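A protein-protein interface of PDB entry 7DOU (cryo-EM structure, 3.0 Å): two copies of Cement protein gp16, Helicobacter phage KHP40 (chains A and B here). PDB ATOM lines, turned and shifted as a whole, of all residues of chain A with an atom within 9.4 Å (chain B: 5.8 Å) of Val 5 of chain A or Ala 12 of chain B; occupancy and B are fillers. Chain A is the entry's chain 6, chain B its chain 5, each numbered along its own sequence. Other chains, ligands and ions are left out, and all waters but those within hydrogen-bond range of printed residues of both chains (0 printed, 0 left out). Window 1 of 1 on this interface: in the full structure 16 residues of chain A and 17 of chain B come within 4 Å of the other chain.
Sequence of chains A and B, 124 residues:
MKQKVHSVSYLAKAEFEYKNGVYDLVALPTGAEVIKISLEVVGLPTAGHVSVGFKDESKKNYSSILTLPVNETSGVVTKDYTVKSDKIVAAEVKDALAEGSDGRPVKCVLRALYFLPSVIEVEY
Among the printed residues, pairs that only touch across the chains: Gln 3 of chain A with Val 26 of chain B (3.4 Å), Val 5 of chain A with Tyr 10 of chain B (3.8 Å), Val 5 of chain A with Leu 11 of chain B (3.5 Å), Val 5 of chain A with Ala 12 of chain B (3.9 Å), Val 5 of chain A with Tyr 114 of chain B (3.8 Å), His 6 of chain A with Tyr 10 of chain B (3.5 Å), Ser 7 of chain A with Tyr 10 of chain B (3.7 Å), Glu 33 of chain A with Leu 11 of chain B (3.8 Å), Glu 33 of chain A with Lys 13 of chain B (2.9 Å), Ile 35 of chain A with Leu 11 of chain B (3.7 Å), Ile 35 of chain A with Leu 113 of chain B (3.7 Å), Phe 115 of chain A with Leu 11 of chain B (3.7 Å), Phe 115 of chain A with Leu 113 of chain B (3.5 Å), Ile 120 of chain A with Tyr 10 of chain B (3.7 Å), Val 122 of chain A with Tyr 10 of chain B (3.8 Å) and Tyr 124 of chain A with Tyr 10 of chain B (3.5 Å).
Of the 20 printed residues of chain A, 11 touch a printed residue of chain B. Printed residues of chain A that touch a printed residue of chain B: Gln 3, Val 5, His 6, Ser 7, Glu 33, Ile 35, Asp 80, Phe 115, Ile 120, Val 122 and Tyr 124. Hydrophobic or aromatic side chains of chain A that line the printed part of chain B: Val 5, His 6, Ile 35, Phe 115, Ile 120, Val 122 and Tyr 124. Hydrophobic or aromatic side chains of chain B within 4 Å of the printed part of chain A: Tyr 10, Leu 11, Ala 12, Val 26, Leu 113 and Tyr 114. Among the printed residues, Asp or Glu carboxylates within 4 Å of a Lys or Arg side-chain nitrogen of the other chain: Glu 33 of chain A with Arg 111 of chain B (2.5 Å).
The backbone carbonyl oxygen of Tyr 114 of chain B lies within hydrogen-bond range of the backbone NH of Tyr 10 of chain B. The backbone carbonyl oxygen of Gln 3 of chain A is in hydrogen-bond range of the backbone NH of Val 122 of chain A (2.9 Å). N of Val 5 of chain A lies within hydrogen-bond range of O of Ile 120 of chain A. ND1 of His 6 of chain A sits at hydrogen-bond distance from O of Leu 116 of chain A, at 3.1 Å. ND1 of His 6 of chain A is in hydrogen-bond range of O of Ser 118 of chain A (3.4 Å). N of Phe 115 of chain A lies within hydrogen-bond range of O of Glu 33 of chain A, 2.7 Å away.
Of chain B, only Tyr 10 (3.8 Å), Leu 11 (3.5 Å), Ala 12 (3.9 Å) and Tyr 114 (3.8 Å) come within 4 Å of Val 5 of chain A. Of the printed residues of chain B, His 6 of chain A touches Tyr 10 and Leu 11. Printed residues of chain B within 4 Å of Phe 115 of chain A: Leu 11 (3.7 Å) and Leu 113 (3.5 Å). Of chain A, only Val 5 (3.5 Å), His 6 (2.7 Å), Glu 33 (3.8 Å), Ile 35 (3.7 Å) and Phe 115 (3.7 Å) come within 4 Å of Leu 11 of chain B. Ala 12 of chain B touches one residue of chain A. No residue of chain A comes within 4 Å of Ala 112 of chain B. The nearest printed residue of chain B that does not touch Val 5 of chain A is Lys 13 of chain B (5.8 Å). The nearest printed residue of chain B that does not touch Glu 33 of chain A is Ala 12 of chain B (7.0 Å).
No position is printed for both chains. Of the 20 pairs that touch across the chains among the printed residues, none has its exchanged pair printed and touching as well.
O of Leu 11 of chain B sits at hydrogen-bond distance from N of His 6 of chain A (2.7 Å). The guanidinium group of Arg 111 of chain B is in salt-bridge range of the side-chain carboxylate of Glu 33 of chain A. O of Asp 80 of chain A is in hydrogen-bond range of NH1 of Arg 111 of chain B (3.4 Å). The side-chain hydroxyl of Tyr 114 of chain B lies within hydrogen-bond range of the side-chain hydroxyl of Tyr 124 of chain A (2.7 Å).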
ATOM      1  N   LYS A   2     -38.140  34.437  32.912  1.00  0.00           N
ATOM      2  CA  LYS A   2     -37.775  33.119  33.408  1.00  0.00           C
ATOM      3  C   LYS A   2     -37.285  32.288  32.237  1.00  0.00           C
ATOM      4  O   LYS A   2     -37.842  32.369  31.139  1.00  0.00           O
ATOM      5  CB  LYS A   2     -38.961  32.429  34.089  1.00  0.00           C
ATOM      6  CG  LYS A   2     -38.580  31.252  34.960  1.00  0.00           C
ATOM      7  CD  LYS A   2     -39.795  30.406  35.287  1.00  0.00           C
ATOM      8  CE  LYS A   2     -40.799  31.180  36.120  1.00  0.00           C
ATOM      9  NZ  LYS A   2     -41.888  30.300  36.626  1.00  0.00           N
ATOM     10  N   GLN A   3     -36.243  31.493  32.467  1.00  0.00           N
ATOM     11  CA  GLN A   3     -35.675  30.704  31.384  1.00  0.00           C
ATOM     12  C   GLN A   3     -34.867  29.556  31.976  1.00  0.00           C
ATOM     13  O   GLN A   3     -34.607  29.507  33.181  1.00  0.00           O
ATOM     14  CB  GLN A   3     -34.821  31.579  30.459  1.00  0.00           C
ATOM     15  CG  GLN A   3     -34.524  30.971  29.102  1.00  0.00           C
ATOM     16  CD  GLN A   3     -33.876  31.957  28.159  1.00  0.00           C
ATOM     17  OE1 GLN A   3     -33.581  33.087  28.537  1.00  0.00           O
ATOM     18  NE2 GLN A   3     -33.658  31.536  26.922  1.00  0.00           N
ATOM     19  N   LYS A   4     -34.499  28.618  31.108  1.00  0.00           N
ATOM     20  CA  LYS A   4     -33.683  27.464  31.457  1.00  0.00           C
ATOM     21  C   LYS A   4     -32.319  27.607  30.795  1.00  0.00           C
ATOM     22  O   LYS A   4     -32.237  27.827  29.582  1.00  0.00           O
ATOM     23  CB  LYS A   4     -34.357  26.168  31.005  1.00  0.00           C
ATOM     24  CG  LYS A   4     -35.592  25.789  31.796  1.00  0.00           C
ATOM     25  CD  LYS A   4     -35.225  25.119  33.104  1.00  0.00           C
ATOM     26  CE  LYS A   4     -36.457  24.579  33.808  1.00  0.00           C
ATOM     27  NZ  LYS A   4     -37.147  23.538  33.000  1.00  0.00           N
ATOM     28  N   VAL A   5     -31.254  27.476  31.587  1.00  0.00           N
ATOM     29  CA  VAL A   5     -29.899  27.704  31.104  1.00  0.00           C
ATOM     30  C   VAL A   5     -28.988  26.566  31.538  1.00  0.00           C
ATOM     31  O   VAL A   5     -29.249  25.858  32.513  1.00  0.00           O
ATOM     32  CB  VAL A   5     -29.327  29.049  31.596  1.00  0.00           C
ATOM     33  CG1 VAL A   5     -30.083  30.209  30.977  1.00  0.00           C
ATOM     34  CG2 VAL A   5     -29.376  29.117  33.109  1.00  0.00           C
ATOM     35  N   HIS A   6     -27.892  26.411  30.799  1.00  0.00           N
ATOM     36  CA  HIS A   6     -26.844  25.457  31.135  1.00  0.00           C
ATOM     37  C   HIS A   6     -25.844  26.138  32.061  1.00  0.00           C
ATOM     38  O   HIS A   6     -25.289  27.186  31.716  1.00  0.00           O
ATOM     39  CB  HIS A   6     -26.145  24.953  29.874  1.00  0.00           C
ATOM     40  CG  HIS A   6     -27.054  24.256  28.913  1.00  0.00           C
ATOM     41  ND1 HIS A   6     -27.618  23.026  29.178  1.00  0.00           N
ATOM     42  CD2 HIS A   6     -27.493  24.614  27.684  1.00  0.00           C
ATOM     43  CE1 HIS A   6     -28.365  22.659  28.154  1.00  0.00           C
ATOM     44  NE2 HIS A   6     -28.309  23.605  27.234  1.00  0.00           N
ATOM     45  N   SER A   7     -25.611  25.542  33.228  1.00  0.00           N
ATOM     46  CA  SER A   7     -24.787  26.157  34.256  1.00  0.00           C
ATOM     47  C   SER A   7     -23.395  25.552  34.376  1.00  0.00           C
ATOM     48  O   SER A   7     -22.545  26.135  35.056  1.00  0.00           O
ATOM     49  CB  SER A   7     -25.489  26.065  35.614  1.00  0.00           C
ATOM     50  OG  SER A   7     -24.611  26.433  36.660  1.00  0.00           O
ATOM     51  N   VAL A   8     -23.136  24.409  33.747  1.00  0.00           N
ATOM     52  CA  VAL A   8     -21.872  23.696  33.887  1.00  0.00           C
ATOM     53  C   VAL A   8     -21.185  23.657  32.531  1.00  0.00           C
ATOM     54  O   VAL A   8     -21.803  23.290  31.526  1.00  0.00           O
ATOM     55  CB  VAL A   8     -22.086  22.277  34.439  1.00  0.00           C
ATOM     56  CG1 VAL A   8     -20.769  21.535  34.510  1.00  0.00           C
ATOM     57  CG2 VAL A   8     -22.737  22.338  35.808  1.00  0.00           C
ATOM     58  N   GLU A  33     -23.472  20.694  24.820  1.00  0.00           N
ATOM     59  CA  GLU A  33     -23.523  21.757  23.824  1.00  0.00           C
ATOM     60  C   GLU A  33     -22.114  22.255  23.551  1.00  0.00           C
ATOM     61  O   GLU A  33     -21.527  22.958  24.378  1.00  0.00           O
ATOM     62  CB  GLU A  33     -24.427  22.894  24.286  1.00  0.00           C
ATOM     63  CG  GLU A  33     -25.879  22.508  24.276  1.00  0.00           C
ATOM     64  CD  GLU A  33     -26.568  22.971  23.021  1.00  0.00           C
ATOM     65  OE1 GLU A  33     -27.770  22.692  22.871  1.00  0.00           O
ATOM     66  OE2 GLU A  33     -25.905  23.609  22.178  1.00  0.00           O
ATOM     67  N   ILE A  35     -19.723  24.732  22.113  1.00  0.00           N
ATOM     68  CA  ILE A  35     -19.708  26.121  21.674  1.00  0.00           C
ATOM     69  C   ILE A  35     -18.357  26.553  21.138  1.00  0.00           C
ATOM     70  O   ILE A  35     -18.267  27.639  20.545  1.00  0.00           O
ATOM     71  CB  ILE A  35     -20.159  27.076  22.797  1.00  0.00           C
ATOM     72  CG1 ILE A  35     -19.373  26.802  24.074  1.00  0.00           C
ATOM     73  CG2 ILE A  35     -21.644  26.924  23.052  1.00  0.00           C
ATOM     74  CD1 ILE A  35     -19.768  27.691  25.219  1.00  0.00           C
ATOM     75  N   ASP A  80     -22.049  25.649  15.841  1.00  0.00           N
ATOM     76  CA  ASP A  80     -22.244  25.046  17.151  1.00  0.00           C
ATOM     77  C   ASP A  80     -23.152  23.830  17.036  1.00  0.00           C
ATOM     78  O   ASP A  80     -24.125  23.827  16.280  1.00  0.00           O
ATOM     79  CB  ASP A  80     -22.837  26.051  18.137  1.00  0.00           C
ATOM     80  CG  ASP A  80     -21.927  27.236  18.375  1.00  0.00           C
ATOM     81  OD1 ASP A  80     -22.157  27.976  19.355  1.00  0.00           O
ATOM     82  OD2 ASP A  80     -20.975  27.424  17.589  1.00  0.00           O
ATOM     83  N   PHE A 115     -20.755  22.908  26.965  1.00  0.00           N
ATOM     84  CA  PHE A 115     -21.600  23.018  28.146  1.00  0.00           C
ATOM     85  C   PHE A 115     -22.306  21.696  28.412  1.00  0.00           C
ATOM     86  O   PHE A 115     -22.717  20.999  27.481  1.00  0.00           O
ATOM     87  CB  PHE A 115     -22.632  24.132  27.979  1.00  0.00           C
ATOM     88  CG  PHE A 115     -22.229  25.428  28.615  1.00  0.00           C
ATOM     89  CD1 PHE A 115     -21.371  26.292  27.967  1.00  0.00           C
ATOM     90  CD2 PHE A 115     -22.710  25.781  29.860  1.00  0.00           C
ATOM     91  CE1 PHE A 115     -21.000  27.482  28.547  1.00  0.00           C
ATOM     92  CE2 PHE A 115     -22.342  26.971  30.445  1.00  0.00           C
ATOM     93  CZ  PHE A 115     -21.487  27.823  29.788  1.00  0.00           C
ATOM     94  N   LEU A 116     -22.442  21.360  29.691  1.00  0.00           N
ATOM     95  CA  LEU A 116     -23.033  20.094  30.084  1.00  0.00           C
ATOM     96  C   LEU A 116     -24.547  20.128  29.888  1.00  0.00           C
ATOM     97  O   LEU A 116     -25.161  21.196  29.907  1.00  0.00           O
ATOM     98  CB  LEU A 116     -22.694  19.783  31.539  1.00  0.00           C
ATOM     99  CG  LEU A 116     -21.371  19.067  31.819  1.00  0.00           C
ATOM    100  CD1 LEU A 116     -21.373  17.670  31.233  1.00  0.00           C
ATOM    101  CD2 LEU A 116     -20.199  19.862  31.286  1.00  0.00           C
ATOM    102  N   PRO A 117     -25.172  18.961  29.696  1.00  0.00           N
ATOM    103  CA  PRO A 117     -26.628  18.931  29.494  1.00  0.00           C
ATOM    104  C   PRO A 117     -27.437  19.336  30.715  1.00  0.00           C
ATOM    105  O   PRO A 117     -28.643  19.573  30.573  1.00  0.00           O
ATOM    106  CB  PRO A 117     -26.895  17.471  29.115  1.00  0.00           C
ATOM    107  CG  PRO A 117     -25.773  16.719  29.731  1.00  0.00           C
ATOM    108  CD  PRO A 117     -24.582  17.616  29.599  1.00  0.00           C
ATOM    109  N   SER A 118     -26.833  19.405  31.898  1.00  0.00           N
ATOM    110  CA  SER A 118     -27.573  19.808  33.086  1.00  0.00           C
ATOM    111  C   SER A 118     -28.099  21.227  32.924  1.00  0.00           C
ATOM    112  O   SER A 118     -27.410  22.109  32.406  1.00  0.00           O
ATOM    113  CB  SER A 118     -26.686  19.711  34.325  1.00  0.00           C
ATOM    114  OG  SER A 118     -27.410  20.051  35.495  1.00  0.00           O
ATOM    115  N   VAL A 119     -29.333  21.446  33.372  1.00  0.00           N
ATOM    116  CA  VAL A 119     -30.049  22.694  33.147  1.00  0.00           C
ATOM    117  C   VAL A 119     -30.653  23.169  34.459  1.00  0.00           C
ATOM    118  O   VAL A 119     -31.197  22.369  35.229  1.00  0.00           O
ATOM    119  CB  VAL A 119     -31.146  22.523  32.075  1.00  0.00           C
ATOM    120  CG1 VAL A 119     -32.000  23.757  31.988  1.00  0.00           C
ATOM    121  CG2 VAL A 119     -30.527  22.234  30.728  1.00  0.00           C
ATOM    122  N   ILE A 120     -30.552  24.472  34.716  1.00  0.00           N
ATOM    123  CA  ILE A 120     -31.183  25.097  35.868  1.00  0.00           C
ATOM    124  C   ILE A 120     -32.131  26.182  35.374  1.00  0.00           C
ATOM    125  O   ILE A 120     -32.096  26.594  34.213  1.00  0.00           O
ATOM    126  CB  ILE A 120     -30.158  25.683  36.857  1.00  0.00           C
ATOM    127  CG1 ILE A 120     -29.309  26.751  36.172  1.00  0.00           C
ATOM    128  CG2 ILE A 120     -29.282  24.583  37.427  1.00  0.00           C
ATOM    129  CD1 ILE A 120     -28.504  27.588  37.132  1.00  0.00           C
ATOM    130  N   GLU A 121     -32.994  26.639  36.275  1.00  0.00           N
ATOM    131  CA  GLU A 121     -33.984  27.660  35.967  1.00  0.00           C
ATOM    132  C   GLU A 121     -33.592  28.972  36.630  1.00  0.00           C
ATOM    133  O   GLU A 121     -33.335  29.008  37.839  1.00  0.00           O
ATOM    134  CB  GLU A 121     -35.374  27.231  36.435  1.00  0.00           C
ATOM    135  CG  GLU A 121     -36.454  28.265  36.184  1.00  0.00           C
ATOM    136  CD  GLU A 121     -37.583  28.183  37.189  1.00  0.00           C
ATOM    137  OE1 GLU A 121     -37.808  29.174  37.915  1.00  0.00           O
ATOM    138  OE2 GLU A 121     -38.245  27.127  37.256  1.00  0.00           O
ATOM    139  N   VAL A 122     -33.550  30.045  35.844  1.00  0.00           N
ATOM    140  CA  VAL A 122     -33.161  31.361  36.333  1.00  0.00           C
ATOM    141  C   VAL A 122     -34.235  32.373  35.958  1.00  0.00           C
ATOM    142  O   VAL A 122     -34.762  32.348  34.839  1.00  0.00           O
ATOM    143  CB  VAL A 122     -31.779  31.791  35.798  1.00  0.00           C
ATOM    144  CG1 VAL A 122     -30.757  30.705  36.058  1.00  0.00           C
ATOM    145  CG2 VAL A 122     -31.836  32.091  34.310  1.00  0.00           C
ATOM    146  N   GLU A 123     -34.581  33.240  36.905  1.00  0.00           N
ATOM    147  CA  GLU A 123     -35.520  34.329  36.678  1.00  0.00           C
ATOM    148  C   GLU A 123     -34.773  35.653  36.754  1.00  0.00           C
ATOM    149  O   GLU A 123     -33.945  35.855  37.648  1.00  0.00           O
ATOM    150  CB  GLU A 123     -36.677  34.295  37.686  1.00  0.00           C
ATOM    151  CG  GLU A 123     -36.325  34.625  39.137  1.00  0.00           C
ATOM    152  CD  GLU A 123     -35.815  33.430  39.925  1.00  0.00           C
ATOM    153  OE1 GLU A 123     -35.445  32.412  39.303  1.00  0.00           O
ATOM    154  OE2 GLU A 123     -35.790  33.510  41.172  1.00  0.00           O
ATOM    155  N   TYR A 124     -35.049  36.539  35.804  1.00  0.00           N
ATOM    156  CA  TYR A 124     -34.399  37.844  35.755  1.00  0.00           C
ATOM    157  C   TYR A 124     -35.415  38.973  35.853  1.00  0.00           C
ATOM    158  O   TYR A 124     -35.670  39.676  34.876  1.00  0.00           O
ATOM    159  CB  TYR A 124     -33.582  37.982  34.472  1.00  0.00           C
ATOM    160  CG  TYR A 124     -32.429  37.011  34.380  1.00  0.00           C
ATOM    161  CD1 TYR A 124     -32.033  36.491  33.159  1.00  0.00           C
ATOM    162  CD2 TYR A 124     -31.727  36.632  35.514  1.00  0.00           C
ATOM    163  CE1 TYR A 124     -30.982  35.604  33.072  1.00  0.00           C
ATOM    164  CE2 TYR A 124     -30.671  35.748  35.434  1.00  0.00           C
ATOM    165  CZ  TYR A 124     -30.303  35.239  34.210  1.00  0.00           C
ATOM    166  OH  TYR A 124     -29.252  34.359  34.121  1.00  0.00           O
ATOM    167  N   TYR B  10     -23.323  31.372  32.007  1.00  0.00           N
ATOM    168  CA  TYR B  10     -24.448  30.560  31.576  1.00  0.00           C
ATOM    169  C   TYR B  10     -24.508  30.504  30.056  1.00  0.00           C
ATOM    170  O   TYR B  10     -24.010  31.396  29.356  1.00  0.00           O
ATOM    171  CB  TYR B  10     -25.779  31.099  32.112  1.00  0.00           C
ATOM    172  CG  TYR B  10     -25.966  30.965  33.604  1.00  0.00           C
ATOM    173  CD1 TYR B  10     -25.229  30.053  34.339  1.00  0.00           C
ATOM    174  CD2 TYR B  10     -26.897  31.743  34.276  1.00  0.00           C
ATOM    175  CE1 TYR B  10     -25.401  29.929  35.701  1.00  0.00           C
ATOM    176  CE2 TYR B  10     -27.075  31.628  35.637  1.00  0.00           C
ATOM    177  CZ  TYR B  10     -26.326  30.719  36.344  1.00  0.00           C
ATOM    178  OH  TYR B  10     -26.503  30.597  37.702  1.00  0.00           O
ATOM    179  N   LEU B  11     -25.108  29.428  29.558  1.00  0.00           N
ATOM    180  CA  LEU B  11     -25.405  29.252  28.145  1.00  0.00           C
ATOM    181  C   LEU B  11     -26.887  28.951  27.996  1.00  0.00           C
ATOM    182  O   LEU B  11     -27.422  28.086  28.696  1.00  0.00           O
ATOM    183  CB  LEU B  11     -24.576  28.123  27.533  1.00  0.00           C
ATOM    184  CG  LEU B  11     -24.809  27.885  26.041  1.00  0.00           C
ATOM    185  CD1 LEU B  11     -23.963  28.826  25.207  1.00  0.00           C
ATOM    186  CD2 LEU B  11     -24.524  26.442  25.679  1.00  0.00           C
ATOM    187  N   ALA B  12     -27.543  29.662  27.087  1.00  0.00           N
ATOM    188  CA  ALA B  12     -28.975  29.529  26.868  1.00  0.00           C
ATOM    189  C   ALA B  12     -29.237  29.082  25.438  1.00  0.00           C
ATOM    190  O   ALA B  12     -28.662  29.636  24.496  1.00  0.00           O
ATOM    191  CB  ALA B  12     -29.700  30.844  27.153  1.00  0.00           C
ATOM    192  N   LYS B  13     -30.101  28.084  25.289  1.00  0.00           N
ATOM    193  CA  LYS B  13     -30.550  27.595  23.993  1.00  0.00           C
ATOM    194  C   LYS B  13     -31.966  28.083  23.734  1.00  0.00           C
ATOM    195  O   LYS B  13     -32.818  28.030  24.627  1.00  0.00           O
ATOM    196  CB  LYS B  13     -30.545  26.069  23.930  1.00  0.00           C
ATOM    197  CG  LYS B  13     -30.922  25.541  22.554  1.00  0.00           C
ATOM    198  CD  LYS B  13     -30.282  24.209  22.257  1.00  0.00           C
ATOM    199  CE  LYS B  13     -30.562  23.234  23.388  1.00  0.00           C
ATOM    200  NZ  LYS B  13     -32.023  23.113  23.652  1.00  0.00           N
ATOM    201  N   ALA B  14     -32.219  28.548  22.517  1.00  0.00           N
ATOM    202  CA  ALA B  14     -33.571  28.842  22.077  1.00  0.00           C
ATOM    203  C   ALA B  14     -33.763  28.318  20.664  1.00  0.00           C
ATOM    204  O   ALA B  14     -32.824  28.283  19.869  1.00  0.00           O
ATOM    205  CB  ALA B  14     -33.867  30.334  22.127  1.00  0.00           C
ATOM    206  N   VAL B  26     -33.694  34.785  24.553  1.00  0.00           N
ATOM    207  CA  VAL B  26     -32.804  34.713  25.706  1.00  0.00           C
ATOM    208  C   VAL B  26     -33.116  35.864  26.648  1.00  0.00           C
ATOM    209  O   VAL B  26     -33.201  37.020  26.220  1.00  0.00           O
ATOM    210  CB  VAL B  26     -31.325  34.744  25.283  1.00  0.00           C
ATOM    211  CG1 VAL B  26     -30.437  34.365  26.452  1.00  0.00           C
ATOM    212  CG2 VAL B  26     -31.089  33.810  24.111  1.00  0.00           C
ATOM    213  N   LEU B 110     -30.574  29.402  18.496  1.00  0.00           N
ATOM    214  CA  LEU B 110     -29.701  30.467  18.963  1.00  0.00           C
ATOM    215  C   LEU B 110     -29.119  30.059  20.306  1.00  0.00           C
ATOM    216  O   LEU B 110     -29.861  29.721  21.235  1.00  0.00           O
ATOM    217  CB  LEU B 110     -30.450  31.800  19.065  1.00  0.00           C
ATOM    218  CG  LEU B 110     -29.635  33.061  19.372  1.00  0.00           C
ATOM    219  CD1 LEU B 110     -30.332  34.276  18.804  1.00  0.00           C
ATOM    220  CD2 LEU B 110     -29.432  33.253  20.862  1.00  0.00           C
ATOM    221  N   ARG B 111     -27.794  30.083  20.393  1.00  0.00           N
ATOM    222  CA  ARG B 111     -27.067  29.787  21.617  1.00  0.00           C
ATOM    223  C   ARG B 111     -26.396  31.061  22.102  1.00  0.00           C
ATOM    224  O   ARG B 111     -25.667  31.712  21.346  1.00  0.00           O
ATOM    225  CB  ARG B 111     -26.027  28.690  21.386  1.00  0.00           C
ATOM    226  CG  ARG B 111     -26.617  27.370  20.938  1.00  0.00           C
ATOM    227  CD  ARG B 111     -25.530  26.391  20.552  1.00  0.00           C
ATOM    228  NE  ARG B 111     -26.078  25.093  20.176  1.00  0.00           N
ATOM    229  CZ  ARG B 111     -26.473  24.777  18.949  1.00  0.00           C
ATOM    230  NH1 ARG B 111     -26.381  25.668  17.972  1.00  0.00           N
ATOM    231  NH2 ARG B 111     -26.960  23.571  18.697  1.00  0.00           N
ATOM    232  N   ALA B 112     -26.647  31.414  23.359  1.00  0.00           N
ATOM    233  CA  ALA B 112     -26.127  32.640  23.949  1.00  0.00           C
ATOM    234  C   ALA B 112     -25.285  32.287  25.162  1.00  0.00           C
ATOM    235  O   ALA B 112     -25.808  31.773  26.155  1.00  0.00           O
ATOM    236  CB  ALA B 112     -27.263  33.586  24.338  1.00  0.00           C
ATOM    237  N   LEU B 113     -23.987  32.552  25.072  1.00  0.00           N
ATOM    238  CA  LEU B 113     -23.054  32.384  26.176  1.00  0.00           C
ATOM    239  C   LEU B 113     -22.773  33.749  26.787  1.00  0.00           C
ATOM    240  O   LEU B 113     -22.234  34.635  26.109  1.00  0.00           O
ATOM    241  CB  LEU B 113     -21.755  31.740  25.699  1.00  0.00           C
ATOM    242  CG  LEU B 113     -20.607  31.771  26.705  1.00  0.00           C
ATOM    243  CD1 LEU B 113     -20.962  30.969  27.932  1.00  0.00           C
ATOM    244  CD2 LEU B 113     -19.329  31.263  26.073  1.00  0.00           C
ATOM    245  N   TYR B 114     -23.127  33.908  28.063  1.00  0.00           N
ATOM    246  CA  TYR B 114     -22.983  35.184  28.747  1.00  0.00           C
ATOM    247  C   TYR B 114     -22.526  34.966  30.180  1.00  0.00           C
ATOM    248  O   TYR B 114     -22.903  33.980  30.819  1.00  0.00           O
ATOM    249  CB  TYR B 114     -24.298  35.978  28.725  1.00  0.00           C
ATOM    250  CG  TYR B 114     -25.430  35.347  29.504  1.00  0.00           C
ATOM    251  CD1 TYR B 114     -25.615  35.628  30.849  1.00  0.00           C
ATOM    252  CD2 TYR B 114     -26.319  34.476  28.891  1.00  0.00           C
ATOM    253  CE1 TYR B 114     -26.645  35.056  31.561  1.00  0.00           C
ATOM    254  CE2 TYR B 114     -27.352  33.901  29.596  1.00  0.00           C
ATOM    255  CZ  TYR B 114     -27.510  34.195  30.931  1.00  0.00           C
ATOM    256  OH  TYR B 114     -28.538  33.626  31.642  1.00  0.00           O
